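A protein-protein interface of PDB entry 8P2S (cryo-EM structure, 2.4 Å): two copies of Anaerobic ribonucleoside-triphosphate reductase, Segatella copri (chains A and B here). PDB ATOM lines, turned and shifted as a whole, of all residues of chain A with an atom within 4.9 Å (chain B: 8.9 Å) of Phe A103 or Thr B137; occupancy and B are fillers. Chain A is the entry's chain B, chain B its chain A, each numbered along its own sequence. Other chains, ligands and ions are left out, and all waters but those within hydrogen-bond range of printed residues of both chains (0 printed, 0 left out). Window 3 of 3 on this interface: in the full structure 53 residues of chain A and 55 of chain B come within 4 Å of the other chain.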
ATOM      1  N   THR A  99      -8.671  11.834  16.508  1.00  0.00           N
ATOM      2  CA  THR A  99      -9.582  12.812  15.921  1.00  0.00           C
ATOM      3  C   THR A  99      -9.770  12.564  14.430  1.00  0.00           C
ATOM      4  O   THR A  99     -10.887  12.681  13.909  1.00  0.00           O
ATOM      5  CB  THR A  99      -9.073  14.232  16.168  1.00  0.00           C
ATOM      6  OG1 THR A  99      -7.729  14.352  15.686  1.00  0.00           O
ATOM      7  CG2 THR A  99      -9.110  14.560  17.651  1.00  0.00           C
ATOM      8  N   ARG A 100      -8.689  12.224  13.723  1.00  0.00           N
ATOM      9  CA  ARG A 100      -8.799  11.927  12.298  1.00  0.00           C
ATOM     10  C   ARG A 100      -9.682  10.711  12.053  1.00  0.00           C
ATOM     11  O   ARG A 100     -10.510  10.711  11.136  1.00  0.00           O
ATOM     12  CB  ARG A 100      -7.412  11.707  11.697  1.00  0.00           C
ATOM     13  CG  ARG A 100      -7.435  11.377  10.214  1.00  0.00           C
ATOM     14  CD  ARG A 100      -6.057  10.998   9.701  1.00  0.00           C
ATOM     15  NE  ARG A 100      -6.056  10.791   8.257  1.00  0.00           N
ATOM     16  CZ  ARG A 100      -6.381   9.653   7.662  1.00  0.00           C
ATOM     17  NH1 ARG A 100      -6.741   8.587   8.358  1.00  0.00           N
ATOM     18  NH2 ARG A 100      -6.346   9.581   6.335  1.00  0.00           N
ATOM     19  N   ASP A 101      -9.516   9.660  12.859  1.00  0.00           N
ATOM     20  CA  ASP A 101     -10.350   8.475  12.697  1.00  0.00           C
ATOM     21  C   ASP A 101     -11.814   8.774  12.994  1.00  0.00           C
ATOM     22  O   ASP A 101     -12.700   8.270  12.295  1.00  0.00           O
ATOM     23  CB  ASP A 101      -9.844   7.342  13.588  1.00  0.00           C
ATOM     24  CG  ASP A 101      -8.703   6.572  12.955  1.00  0.00           C
ATOM     25  OD1 ASP A 101      -7.579   7.111  12.892  1.00  0.00           O
ATOM     26  OD2 ASP A 101      -8.931   5.425  12.515  1.00  0.00           O
ATOM     27  N   VAL A 102     -12.087   9.589  14.016  1.00  0.00           N
ATOM     28  CA  VAL A 102     -13.469   9.966  14.297  1.00  0.00           C
ATOM     29  C   VAL A 102     -14.055  10.781  13.150  1.00  0.00           C
ATOM     30  O   VAL A 102     -15.208  10.568  12.755  1.00  0.00           O
ATOM     31  CB  VAL A 102     -13.564  10.725  15.634  1.00  0.00           C
ATOM     32  CG1 VAL A 102     -14.978  11.228  15.852  1.00  0.00           C
ATOM     33  CG2 VAL A 102     -13.146   9.825  16.784  1.00  0.00           C
ATOM     34  N   PHE A 103     -13.283  11.712  12.588  1.00  0.00           N
ATOM     35  CA  PHE A 103     -13.764  12.543  11.492  1.00  0.00           C
ATOM     36  C   PHE A 103     -13.864  11.796  10.169  1.00  0.00           C
ATOM     37  O   PHE A 103     -14.575  12.259   9.273  1.00  0.00           O
ATOM     38  CB  PHE A 103     -12.857  13.764  11.310  1.00  0.00           C
ATOM     39  CG  PHE A 103     -13.004  14.792  12.390  1.00  0.00           C
ATOM     40  CD1 PHE A 103     -14.226  14.996  13.007  1.00  0.00           C
ATOM     41  CD2 PHE A 103     -11.919  15.552  12.794  1.00  0.00           C
ATOM     42  CE1 PHE A 103     -14.366  15.942  14.003  1.00  0.00           C
ATOM     43  CE2 PHE A 103     -12.053  16.500  13.790  1.00  0.00           C
ATOM     44  CZ  PHE A 103     -13.277  16.694  14.396  1.00  0.00           C
ATOM     45  N   MET A 104     -13.180  10.664  10.025  1.00  0.00           N
ATOM     46  CA  MET A 104     -13.310   9.846   8.825  1.00  0.00           C
ATOM     47  C   MET A 104     -14.366   8.761   8.952  1.00  0.00           C
ATOM     48  O   MET A 104     -14.894   8.306   7.933  1.00  0.00           O
ATOM     49  CB  MET A 104     -11.967   9.202   8.467  1.00  0.00           C
ATOM     50  CG  MET A 104     -10.918  10.189   7.988  1.00  0.00           C
ATOM     51  SD  MET A 104     -10.232   9.762   6.377  1.00  0.00           S
ATOM     52  CE  MET A 104     -11.675   9.939   5.332  1.00  0.00           C
ATOM     53  N   SER A 105     -14.685   8.332  10.176  1.00  0.00           N
ATOM     54  CA  SER A 105     -15.817   7.432  10.366  1.00  0.00           C
ATOM     55  C   SER A 105     -17.120   8.106   9.956  1.00  0.00           C
ATOM     56  O   SER A 105     -18.018   7.459   9.403  1.00  0.00           O
ATOM     57  CB  SER A 105     -15.885   6.975  11.822  1.00  0.00           C
ATOM     58  OG  SER A 105     -15.979   8.087  12.694  1.00  0.00           O
ATOM     59  N   ILE A 106     -17.245   9.404  10.237  1.00  0.00           N
ATOM     60  CA  ILE A 106     -18.402  10.168   9.781  1.00  0.00           C
ATOM     61  C   ILE A 106     -18.415  10.256   8.260  1.00  0.00           C
ATOM     62  O   ILE A 106     -19.469  10.129   7.624  1.00  0.00           O
ATOM     63  CB  ILE A 106     -18.402  11.564  10.431  1.00  0.00           C
ATOM     64  CG1 ILE A 106     -18.333  11.436  11.953  1.00  0.00           C
ATOM     65  CG2 ILE A 106     -19.635  12.347  10.015  1.00  0.00           C
ATOM     66  CD1 ILE A 106     -18.102  12.745  12.673  1.00  0.00           C
ATOM     67  N   VAL A 107     -17.245  10.476   7.654  1.00  0.00           N
ATOM     68  CA  VAL A 107     -17.163  10.608   6.204  1.00  0.00           C
ATOM     69  C   VAL A 107     -17.561   9.307   5.518  1.00  0.00           C
ATOM     70  O   VAL A 107     -18.310   9.313   4.534  1.00  0.00           O
ATOM     71  CB  VAL A 107     -15.749  11.056   5.789  1.00  0.00           C
ATOM     72  CG1 VAL A 107     -15.576  10.957   4.284  1.00  0.00           C
ATOM     73  CG2 VAL A 107     -15.487  12.472   6.254  1.00  0.00           C
ATOM     74  N   PHE A 133     -19.795  16.536  12.713  1.00  0.00           N
ATOM     75  CA  PHE A 133     -18.529  17.249  12.868  1.00  0.00           C
ATOM     76  C   PHE A 133     -18.643  18.350  13.913  1.00  0.00           C
ATOM     77  O   PHE A 133     -17.737  18.537  14.734  1.00  0.00           O
ATOM     78  CB  PHE A 133     -18.079  17.825  11.525  1.00  0.00           C
ATOM     79  CG  PHE A 133     -17.648  16.786  10.533  1.00  0.00           C
ATOM     80  CD1 PHE A 133     -16.951  15.663  10.944  1.00  0.00           C
ATOM     81  CD2 PHE A 133     -17.949  16.924   9.191  1.00  0.00           C
ATOM     82  CE1 PHE A 133     -16.557  14.705  10.032  1.00  0.00           C
ATOM     83  CE2 PHE A 133     -17.558  15.971   8.275  1.00  0.00           C
ATOM     84  CZ  PHE A 133     -16.863  14.858   8.696  1.00  0.00           C
ATOM     85  N   ALA A 134     -19.756  19.086  13.903  1.00  0.00           N
ATOM     86  CA  ALA A 134     -19.970  20.112  14.918  1.00  0.00           C
ATOM     87  C   ALA A 134     -20.046  19.502  16.312  1.00  0.00           C
ATOM     88  O   ALA A 134     -19.487  20.049  17.269  1.00  0.00           O
ATOM     89  CB  ALA A 134     -21.238  20.905  14.607  1.00  0.00           C
ATOM     90  N   GLU A 136     -18.636  16.703  17.333  1.00  0.00           N
ATOM     91  CA  GLU A 136     -17.323  16.207  17.720  1.00  0.00           C
ATOM     92  C   GLU A 136     -16.349  17.340  18.015  1.00  0.00           C
ATOM     93  O   GLU A 136     -15.406  17.152  18.790  1.00  0.00           O
ATOM     94  CB  GLU A 136     -16.765  15.292  16.633  1.00  0.00           C
ATOM     95  CG  GLU A 136     -15.467  14.595  17.014  1.00  0.00           C
ATOM     96  CD  GLU A 136     -15.616  13.695  18.227  1.00  0.00           C
ATOM     97  OE1 GLU A 136     -16.720  13.150  18.438  1.00  0.00           O
ATOM     98  OE2 GLU A 136     -14.626  13.533  18.971  1.00  0.00           O
ATOM     99  N   THR A 137     -16.541  18.511  17.412  1.00  0.00           N
ATOM    100  CA  THR A 137     -15.693  19.647  17.755  1.00  0.00           C
ATOM    101  C   THR A 137     -16.219  20.453  18.935  1.00  0.00           C
ATOM    102  O   THR A 137     -15.476  21.278  19.476  1.00  0.00           O
ATOM    103  CB  THR A 137     -15.516  20.581  16.551  1.00  0.00           C
ATOM    104  OG1 THR A 137     -14.528  21.571  16.859  1.00  0.00           O
ATOM    105  CG2 THR A 137     -16.814  21.284  16.219  1.00  0.00           C
ATOM    106  N   MET B 129     -24.120  28.840  14.617  1.00  0.00           N
ATOM    107  CA  MET B 129     -22.927  28.488  15.378  1.00  0.00           C
ATOM    108  C   MET B 129     -22.501  27.052  15.103  1.00  0.00           C
ATOM    109  O   MET B 129     -21.306  26.763  14.980  1.00  0.00           O
ATOM    110  CB  MET B 129     -23.179  28.698  16.868  1.00  0.00           C
ATOM    111  CG  MET B 129     -23.394  30.145  17.260  1.00  0.00           C
ATOM    112  SD  MET B 129     -23.637  30.340  19.034  1.00  0.00           S
ATOM    113  CE  MET B 129     -23.776  32.119  19.165  1.00  0.00           C
ATOM    114  N   MET B 130     -23.467  26.136  15.016  1.00  0.00           N
ATOM    115  CA  MET B 130     -23.141  24.743  14.727  1.00  0.00           C
ATOM    116  C   MET B 130     -22.493  24.607  13.357  1.00  0.00           C
ATOM    117  O   MET B 130     -21.502  23.883  13.194  1.00  0.00           O
ATOM    118  CB  MET B 130     -24.400  23.882  14.819  1.00  0.00           C
ATOM    119  CG  MET B 130     -24.875  23.607  16.235  1.00  0.00           C
ATOM    120  SD  MET B 130     -23.742  22.567  17.177  1.00  0.00           S
ATOM    121  CE  MET B 130     -22.880  23.794  18.151  1.00  0.00           C
ATOM    122  N   MET B 131     -23.034  25.304  12.357  1.00  0.00           N
ATOM    123  CA  MET B 131     -22.438  25.243  11.027  1.00  0.00           C
ATOM    124  C   MET B 131     -21.060  25.892  11.001  1.00  0.00           C
ATOM    125  O   MET B 131     -20.165  25.428  10.288  1.00  0.00           O
ATOM    126  CB  MET B 131     -23.361  25.891  10.000  1.00  0.00           C
ATOM    127  CG  MET B 131     -24.275  24.901   9.313  1.00  0.00           C
ATOM    128  SD  MET B 131     -23.372  23.581   8.484  1.00  0.00           S
ATOM    129  CE  MET B 131     -22.270  24.534   7.442  1.00  0.00           C
ATOM    130  N   LYS B 132     -20.871  26.970  11.764  1.00  0.00           N
ATOM    131  CA  LYS B 132     -19.552  27.589  11.849  1.00  0.00           C
ATOM    132  C   LYS B 132     -18.536  26.633  12.462  1.00  0.00           C
ATOM    133  O   LYS B 132     -17.406  26.514  11.971  1.00  0.00           O
ATOM    134  CB  LYS B 132     -19.636  28.882  12.656  1.00  0.00           C
ATOM    135  CG  LYS B 132     -18.298  29.542  12.918  1.00  0.00           C
ATOM    136  CD  LYS B 132     -18.461  30.803  13.751  1.00  0.00           C
ATOM    137  CE  LYS B 132     -19.200  30.516  15.051  1.00  0.00           C
ATOM    138  NZ  LYS B 132     -18.491  29.508  15.886  1.00  0.00           N
ATOM    139  N   PHE B 133     -18.925  25.934  13.530  1.00  0.00           N
ATOM    140  CA  PHE B 133     -18.039  24.944  14.138  1.00  0.00           C
ATOM    141  C   PHE B 133     -17.721  23.821  13.160  1.00  0.00           C
ATOM    142  O   PHE B 133     -16.573  23.370  13.061  1.00  0.00           O
ATOM    143  CB  PHE B 133     -18.673  24.387  15.413  1.00  0.00           C
ATOM    144  CG  PHE B 133     -18.668  25.347  16.565  1.00  0.00           C
ATOM    145  CD1 PHE B 133     -17.553  26.120  16.837  1.00  0.00           C
ATOM    146  CD2 PHE B 133     -19.781  25.483  17.374  1.00  0.00           C
ATOM    147  CE1 PHE B 133     -17.549  27.003  17.898  1.00  0.00           C
ATOM    148  CE2 PHE B 133     -19.783  26.363  18.434  1.00  0.00           C
ATOM    149  CZ  PHE B 133     -18.666  27.125  18.696  1.00  0.00           C
ATOM    150  N   ALA B 134     -18.733  23.355  12.425  1.00  0.00           N
ATOM    151  CA  ALA B 134     -18.509  22.294  11.448  1.00  0.00           C
ATOM    152  C   ALA B 134     -17.548  22.742  10.351  1.00  0.00           C
ATOM    153  O   ALA B 134     -16.663  21.985   9.943  1.00  0.00           O
ATOM    154  CB  ALA B 134     -19.840  21.845  10.852  1.00  0.00           C
ATOM    155  N   SER B 135     -17.707  23.973   9.861  1.00  0.00           N
ATOM    156  CA  SER B 135     -16.795  24.481   8.840  1.00  0.00           C
ATOM    157  C   SER B 135     -15.378  24.615   9.383  1.00  0.00           C
ATOM    158  O   SER B 135     -14.404  24.278   8.693  1.00  0.00           O
ATOM    159  CB  SER B 135     -17.298  25.825   8.312  1.00  0.00           C
ATOM    160  OG  SER B 135     -16.425  26.342   7.323  1.00  0.00           O
ATOM    161  N   GLU B 136     -15.242  25.101  10.620  1.00  0.00           N
ATOM    162  CA  GLU B 136     -13.919  25.285  11.204  1.00  0.00           C
ATOM    163  C   GLU B 136     -13.251  23.957  11.532  1.00  0.00           C
ATOM    164  O   GLU B 136     -12.024  23.902  11.659  1.00  0.00           O
ATOM    165  CB  GLU B 136     -14.015  26.153  12.457  1.00  0.00           C
ATOM    166  CG  GLU B 136     -14.392  27.596  12.178  1.00  0.00           C
ATOM    167  CD  GLU B 136     -14.513  28.421  13.445  1.00  0.00           C
ATOM    168  OE1 GLU B 136     -14.311  27.860  14.542  1.00  0.00           O
ATOM    169  OE2 GLU B 136     -14.811  29.629  13.343  1.00  0.00           O
ATOM    170  N   THR B 137     -14.026  22.888  11.692  1.00  0.00           N
ATOM    171  CA  THR B 137     -13.417  21.578  11.886  1.00  0.00           C
ATOM    172  C   THR B 137     -13.280  20.780  10.595  1.00  0.00           C
ATOM    173  O   THR B 137     -12.598  19.749  10.598  1.00  0.00           O
ATOM    174  CB  THR B 137     -14.211  20.754  12.906  1.00  0.00           C
ATOM    175  OG1 THR B 137     -13.459  19.587  13.258  1.00  0.00           O
ATOM    176  CG2 THR B 137     -15.536  20.317  12.327  1.00  0.00           C
ATOM    177  N   THR B 138     -13.903  21.217   9.500  1.00  0.00           N
ATOM    178  CA  THR B 138     -13.755  20.534   8.218  1.00  0.00           C
ATOM    179  C   THR B 138     -12.677  21.133   7.327  1.00  0.00           C
ATOM    180  O   THR B 138     -11.918  20.381   6.710  1.00  0.00           O
ATOM    181  CB  THR B 138     -15.079  20.527   7.447  1.00  0.00           C
ATOM    182  OG1 THR B 138     -15.667  21.833   7.485  1.00  0.00           O
ATOM    183  CG2 THR B 138     -16.035  19.520   8.040  1.00  0.00           C
ATOM    184  N   LYS B 139     -12.592  22.463   7.228  1.00  0.00           N
ATOM    185  CA  LYS B 139     -11.613  23.066   6.323  1.00  0.00           C
ATOM    186  C   LYS B 139     -10.179  22.665   6.657  1.00  0.00           C
ATOM    187  O   LYS B 139      -9.442  22.262   5.736  1.00  0.00           O
ATOM    188  CB  LYS B 139     -11.791  24.589   6.304  1.00  0.00           C
ATOM    189  CG  LYS B 139     -13.114  25.048   5.719  1.00  0.00           C
ATOM    190  CD  LYS B 139     -13.274  26.555   5.813  1.00  0.00           C
ATOM    191  CE  LYS B 139     -12.211  27.278   5.005  1.00  0.00           C
ATOM    192  NZ  LYS B 139     -12.384  28.756   5.058  1.00  0.00           N
ATOM    193  N   PRO B 140      -9.714  22.737   7.911  1.00  0.00           N
ATOM    194  CA  PRO B 140      -8.385  22.181   8.205  1.00  0.00           C
ATOM    195  C   PRO B 140      -8.280  20.704   7.887  1.00  0.00           C
ATOM    196  O   PRO B 140      -7.205  20.237   7.493  1.00  0.00           O
ATOM    197  CB  PRO B 140      -8.219  22.457   9.705  1.00  0.00           C
ATOM    198  CG  PRO B 140      -9.098  23.616   9.969  1.00  0.00           C
ATOM    199  CD  PRO B 140     -10.287  23.406   9.092  1.00  0.00           C
ATOM    200  N   PHE B 141      -9.368  19.950   8.045  1.00  0.00           N
ATOM    201  CA  PHE B 141      -9.305  18.519   7.772  1.00  0.00           C
ATOM    202  C   PHE B 141      -9.137  18.249   6.284  1.00  0.00           C
ATOM    203  O   PHE B 141      -8.319  17.416   5.890  1.00  0.00           O
ATOM    204  CB  PHE B 141     -10.544  17.804   8.300  1.00  0.00           C
ATOM    205  CG  PHE B 141     -10.583  16.348   7.938  1.00  0.00           C
ATOM    206  CD1 PHE B 141      -9.761  15.442   8.584  1.00  0.00           C
ATOM    207  CD2 PHE B 141     -11.424  15.887   6.941  1.00  0.00           C
ATOM    208  CE1 PHE B 141      -9.784  14.103   8.251  1.00  0.00           C
ATOM    209  CE2 PHE B 141     -11.450  14.547   6.604  1.00  0.00           C
ATOM    210  CZ  PHE B 141     -10.628  13.655   7.260  1.00  0.00           C
ATOM    211  N   VAL B 142      -9.915  18.927   5.437  1.00  0.00           N
ATOM    212  CA  VAL B 142      -9.768  18.715   3.999  1.00  0.00           C
ATOM    213  C   VAL B 142      -8.406  19.210   3.530  1.00  0.00           C
ATOM    214  O   VAL B 142      -7.803  18.639   2.612  1.00  0.00           O
ATOM    215  CB  VAL B 142     -10.924  19.372   3.218  1.00  0.00           C
ATOM    216  CG1 VAL B 142     -11.109  20.806   3.625  1.00  0.00           C
ATOM    217  CG2 VAL B 142     -10.665  19.293   1.730  1.00  0.00           C
ATOM    218  N   ASP B 143      -7.879  20.257   4.174  1.00  0.00           N
ATOM    219  CA  ASP B 143      -6.534  20.713   3.837  1.00  0.00           C
ATOM    220  C   ASP B 143      -5.476  19.640   4.081  1.00  0.00           C
ATOM    221  O   ASP B 143      -4.370  19.744   3.540  1.00  0.00           O
ATOM    222  CB  ASP B 143      -6.188  21.972   4.633  1.00  0.00           C
ATOM    223  CG  ASP B 143      -6.931  23.197   4.139  1.00  0.00           C
ATOM    224  OD1 ASP B 143      -7.738  23.063   3.197  1.00  0.00           O
ATOM    225  OD2 ASP B 143      -6.708  24.294   4.692  1.00  0.00           O
ATOM    226  N   TYR B 145      -4.498  15.372   4.185  1.00  0.00           N
ATOM    227  CA  TYR B 145      -4.788  13.988   3.808  1.00  0.00           C
ATOM    228  C   TYR B 145      -5.727  13.887   2.609  1.00  0.00           C
ATOM    229  O   TYR B 145      -5.936  12.792   2.077  1.00  0.00           O
ATOM    230  CB  TYR B 145      -5.393  13.194   4.974  1.00  0.00           C
ATOM    231  CG  TYR B 145      -4.863  13.544   6.345  1.00  0.00           C
ATOM    232  CD1 TYR B 145      -3.541  13.298   6.686  1.00  0.00           C
ATOM    233  CD2 TYR B 145      -5.697  14.102   7.305  1.00  0.00           C
ATOM    234  CE1 TYR B 145      -3.061  13.613   7.942  1.00  0.00           C
ATOM    235  CE2 TYR B 145      -5.227  14.420   8.560  1.00  0.00           C
ATOM    236  CZ  TYR B 145      -3.909  14.174   8.875  1.00  0.00           C
ATOM    237  OH  TYR B 145      -3.435  14.490  10.127  1.00  0.00           O
ATOM    238  N   LEU B 146      -6.298  15.009   2.173  1.00  0.00           N
ATOM    239  CA  LEU B 146      -7.208  15.018   1.031  1.00  0.00           C
ATOM    240  C   LEU B 146      -6.662  15.846  -0.122  1.00  0.00           C
ATOM    241  O   LEU B 146      -6.597  15.349  -1.251  1.00  0.00           O
ATOM    242  CB  LEU B 146      -8.591  15.526   1.456  1.00  0.00           C
ATOM    243  CG  LEU B 146      -9.414  14.585   2.339  1.00  0.00           C
ATOM    244  CD1 LEU B 146     -10.783  15.173   2.619  1.00  0.00           C
ATOM    245  CD2 LEU B 146      -9.541  13.224   1.687  1.00  0.00           C
ATOM    246  N   LYS B 165     -15.059  24.487   0.442  1.00  0.00           N
ATOM    247  CA  LYS B 165     -14.047  23.607   1.017  1.00  0.00           C
ATOM    248  C   LYS B 165     -14.608  22.867   2.223  1.00  0.00           C
ATOM    249  O   LYS B 165     -14.294  21.693   2.444  1.00  0.00           O
ATOM    250  CB  LYS B 165     -12.800  24.406   1.390  1.00  0.00           C
ATOM    251  CG  LYS B 165     -11.518  23.590   1.360  1.00  0.00           C
ATOM    252  CD  LYS B 165     -10.287  24.474   1.425  1.00  0.00           C
ATOM    253  CE  LYS B 165     -10.230  25.248   2.725  1.00  0.00           C
ATOM    254  NZ  LYS B 165      -9.032  26.129   2.794  1.00  0.00           N
ATOM    255  N   ASP B 166     -15.417  23.545   3.031  1.00  0.00           N
ATOM    256  CA  ASP B 166     -16.355  22.836   3.884  1.00  0.00           C
ATOM    257  C   ASP B 166     -17.436  22.210   3.011  1.00  0.00           C
ATOM    258  O   ASP B 166     -17.854  22.788   2.006  1.00  0.00           O
ATOM    259  CB  ASP B 166     -16.971  23.783   4.910  1.00  0.00           C
ATOM    260  CG  ASP B 166     -17.596  25.006   4.271  1.00  0.00           C
ATOM    261  OD1 ASP B 166     -17.095  25.448   3.216  1.00  0.00           O
ATOM    262  OD2 ASP B 166     -18.587  25.526   4.825  1.00  0.00           O
ATOM    263  N   TYR B 167     -17.887  21.023   3.410  1.00  0.00           N
ATOM    264  CA  TYR B 167     -18.712  20.072   2.656  1.00  0.00           C
ATOM    265  C   TYR B 167     -17.867  19.240   1.698  1.00  0.00           C
ATOM    266  O   TYR B 167     -18.420  18.362   1.023  1.00  0.00           O
ATOM    267  CB  TYR B 167     -19.853  20.718   1.853  1.00  0.00           C
ATOM    268  CG  TYR B 167     -20.917  21.395   2.684  1.00  0.00           C
ATOM    269  CD1 TYR B 167     -22.022  20.689   3.137  1.00  0.00           C
ATOM    270  CD2 TYR B 167     -20.826  22.743   3.002  1.00  0.00           C
ATOM    271  CE1 TYR B 167     -22.999  21.302   3.890  1.00  0.00           C
ATOM    272  CE2 TYR B 167     -21.799  23.365   3.756  1.00  0.00           C
ATOM    273  CZ  TYR B 167     -22.883  22.641   4.198  1.00  0.00           C
ATOM    274  OH  TYR B 167     -23.858  23.252   4.949  1.00  0.00           O
ATOM    275  N   PRO B 169     -15.608  16.962   2.791  1.00  0.00           N
ATOM    276  CA  PRO B 169     -15.703  15.593   3.325  1.00  0.00           C
ATOM    277  C   PRO B 169     -17.045  14.937   3.071  1.00  0.00           C
ATOM    278  O   PRO B 169     -17.133  13.704   3.114  1.00  0.00           O
ATOM    279  CB  PRO B 169     -15.452  15.782   4.827  1.00  0.00           C
ATOM    280  CG  PRO B 169     -14.725  17.065   4.931  1.00  0.00           C
ATOM    281  CD  PRO B 169     -15.296  17.926   3.862  1.00  0.00           C
ATOM    282  N   THR B 170     -18.091  15.718   2.813  1.00  0.00           N
ATOM    283  CA  THR B 170     -19.421  15.180   2.577  1.00  0.00           C
ATOM    284  C   THR B 170     -19.600  14.625   1.172  1.00  0.00           C
ATOM    285  O   THR B 170     -20.642  14.019   0.897  1.00  0.00           O
ATOM    286  CB  THR B 170     -20.473  16.260   2.829  1.00  0.00           C
ATOM    287  OG1 THR B 170     -20.337  17.297   1.851  1.00  0.00           O
ATOM    288  CG2 THR B 170     -20.294  16.861   4.212  1.00  0.00           C
ATOM    289  N   PHE B 488     -12.807  11.762  -5.406  1.00  0.00           N
ATOM    290  CA  PHE B 488     -13.297  11.607  -4.042  1.00  0.00           C
ATOM    291  C   PHE B 488     -14.820  11.528  -4.003  1.00  0.00           C
ATOM    292  O   PHE B 488     -15.386  10.723  -3.255  1.00  0.00           O
ATOM    293  CB  PHE B 488     -12.792  12.761  -3.176  1.00  0.00           C
ATOM    294  CG  PHE B 488     -13.109  12.611  -1.719  1.00  0.00           C
ATOM    295  CD1 PHE B 488     -12.598  11.551  -0.992  1.00  0.00           C
ATOM    296  CD2 PHE B 488     -13.902  13.538  -1.070  1.00  0.00           C
ATOM    297  CE1 PHE B 488     -12.883  11.413   0.349  1.00  0.00           C
ATOM    298  CE2 PHE B 488     -14.189  13.407   0.272  1.00  0.00           C
ATOM    299  CZ  PHE B 488     -13.679  12.343   0.982  1.00  0.00           C
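Of chain B, only Thr B137 (3.1 Å) comes within 4 Å of Phe A103.
No residue of chain B comes within 4 Å of Val A102.
Of the printed residues of chain B, Val A107 touches Pro B169 (3.4 Å).
Of the printed residues of chain B, Ala A134 touches Met B130.
Printed residues of chain B within 4 Å of Thr A137: Phe B133 and Thr B137.
Printed residues of chain A within 4 Å of Phe B133: Thr A137 (3.7 Å).
Printed residues of chain A within 4 Å of Met B130: Ala A134.
Ala B134 touches none of the printed residues of chain A.
The nearest residue of chain A that does not touch Thr B137 is Ala A134 (4.7 Å).
Of the 13 printed residues of chain A, 7 touch a printed residue of chain B.
Printed residues of chain A that touch a printed residue of chain B: Arg A100, Phe A103, Met A104, Val A107, Phe A133, Ala A134 and Thr A137.
Printed residues of chain B that touch a printed residue of chain A: Met B130, Phe B133, Thr B137, Thr B138, Phe B141, Tyr B145 and Pro B169.
Along chain B the printed residues that touch a printed residue of chain A span positions 130 to 169.
Among the printed residues, 9 pairs touch across the chains.
Among the printed residues, no Asp or Glu carboxylate lies within 4 Å of a Lys or Arg side-chain nitrogen of the other chain.
The backbone carbonyl oxygen of Ala B134 lies within hydrogen-bond range of the side-chain hydroxyl of Thr B138 (2.7 Å).
The backbone carbonyl oxygen (O) of Ser B135 sits at hydrogen-bond distance from the side-chain hydroxyl (OG1) of Thr B138, 3.0 Å away.
Phe A133 touches Thr B137, and with the chains exchanged Thr A137 touches Phe B133.
Thr B137 touches its own counterpart, Thr A137.
Tyr B145 touches Arg A100 (CD2 to NE, 3.5 Å).
Thr B137 touches Phe A103 (OG1 to CZ, 3.1 Å).
CZ of Phe B141 touches CG of Met A104 (3.6 Å).
Val A107 touches Pro B169.
Phe A133 touches Thr B137 (CB to CG2, 3.6 Å).
Phe A133 touches Thr B138 (CD2 to CG2, 3.4 Å).
Ala A134 touches Met B130 (CB to O, 3.3 Å).
CG2 of Thr A137 touches CB of Phe B133, at 3.7 Å.
Thr B137 touches Thr A137.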
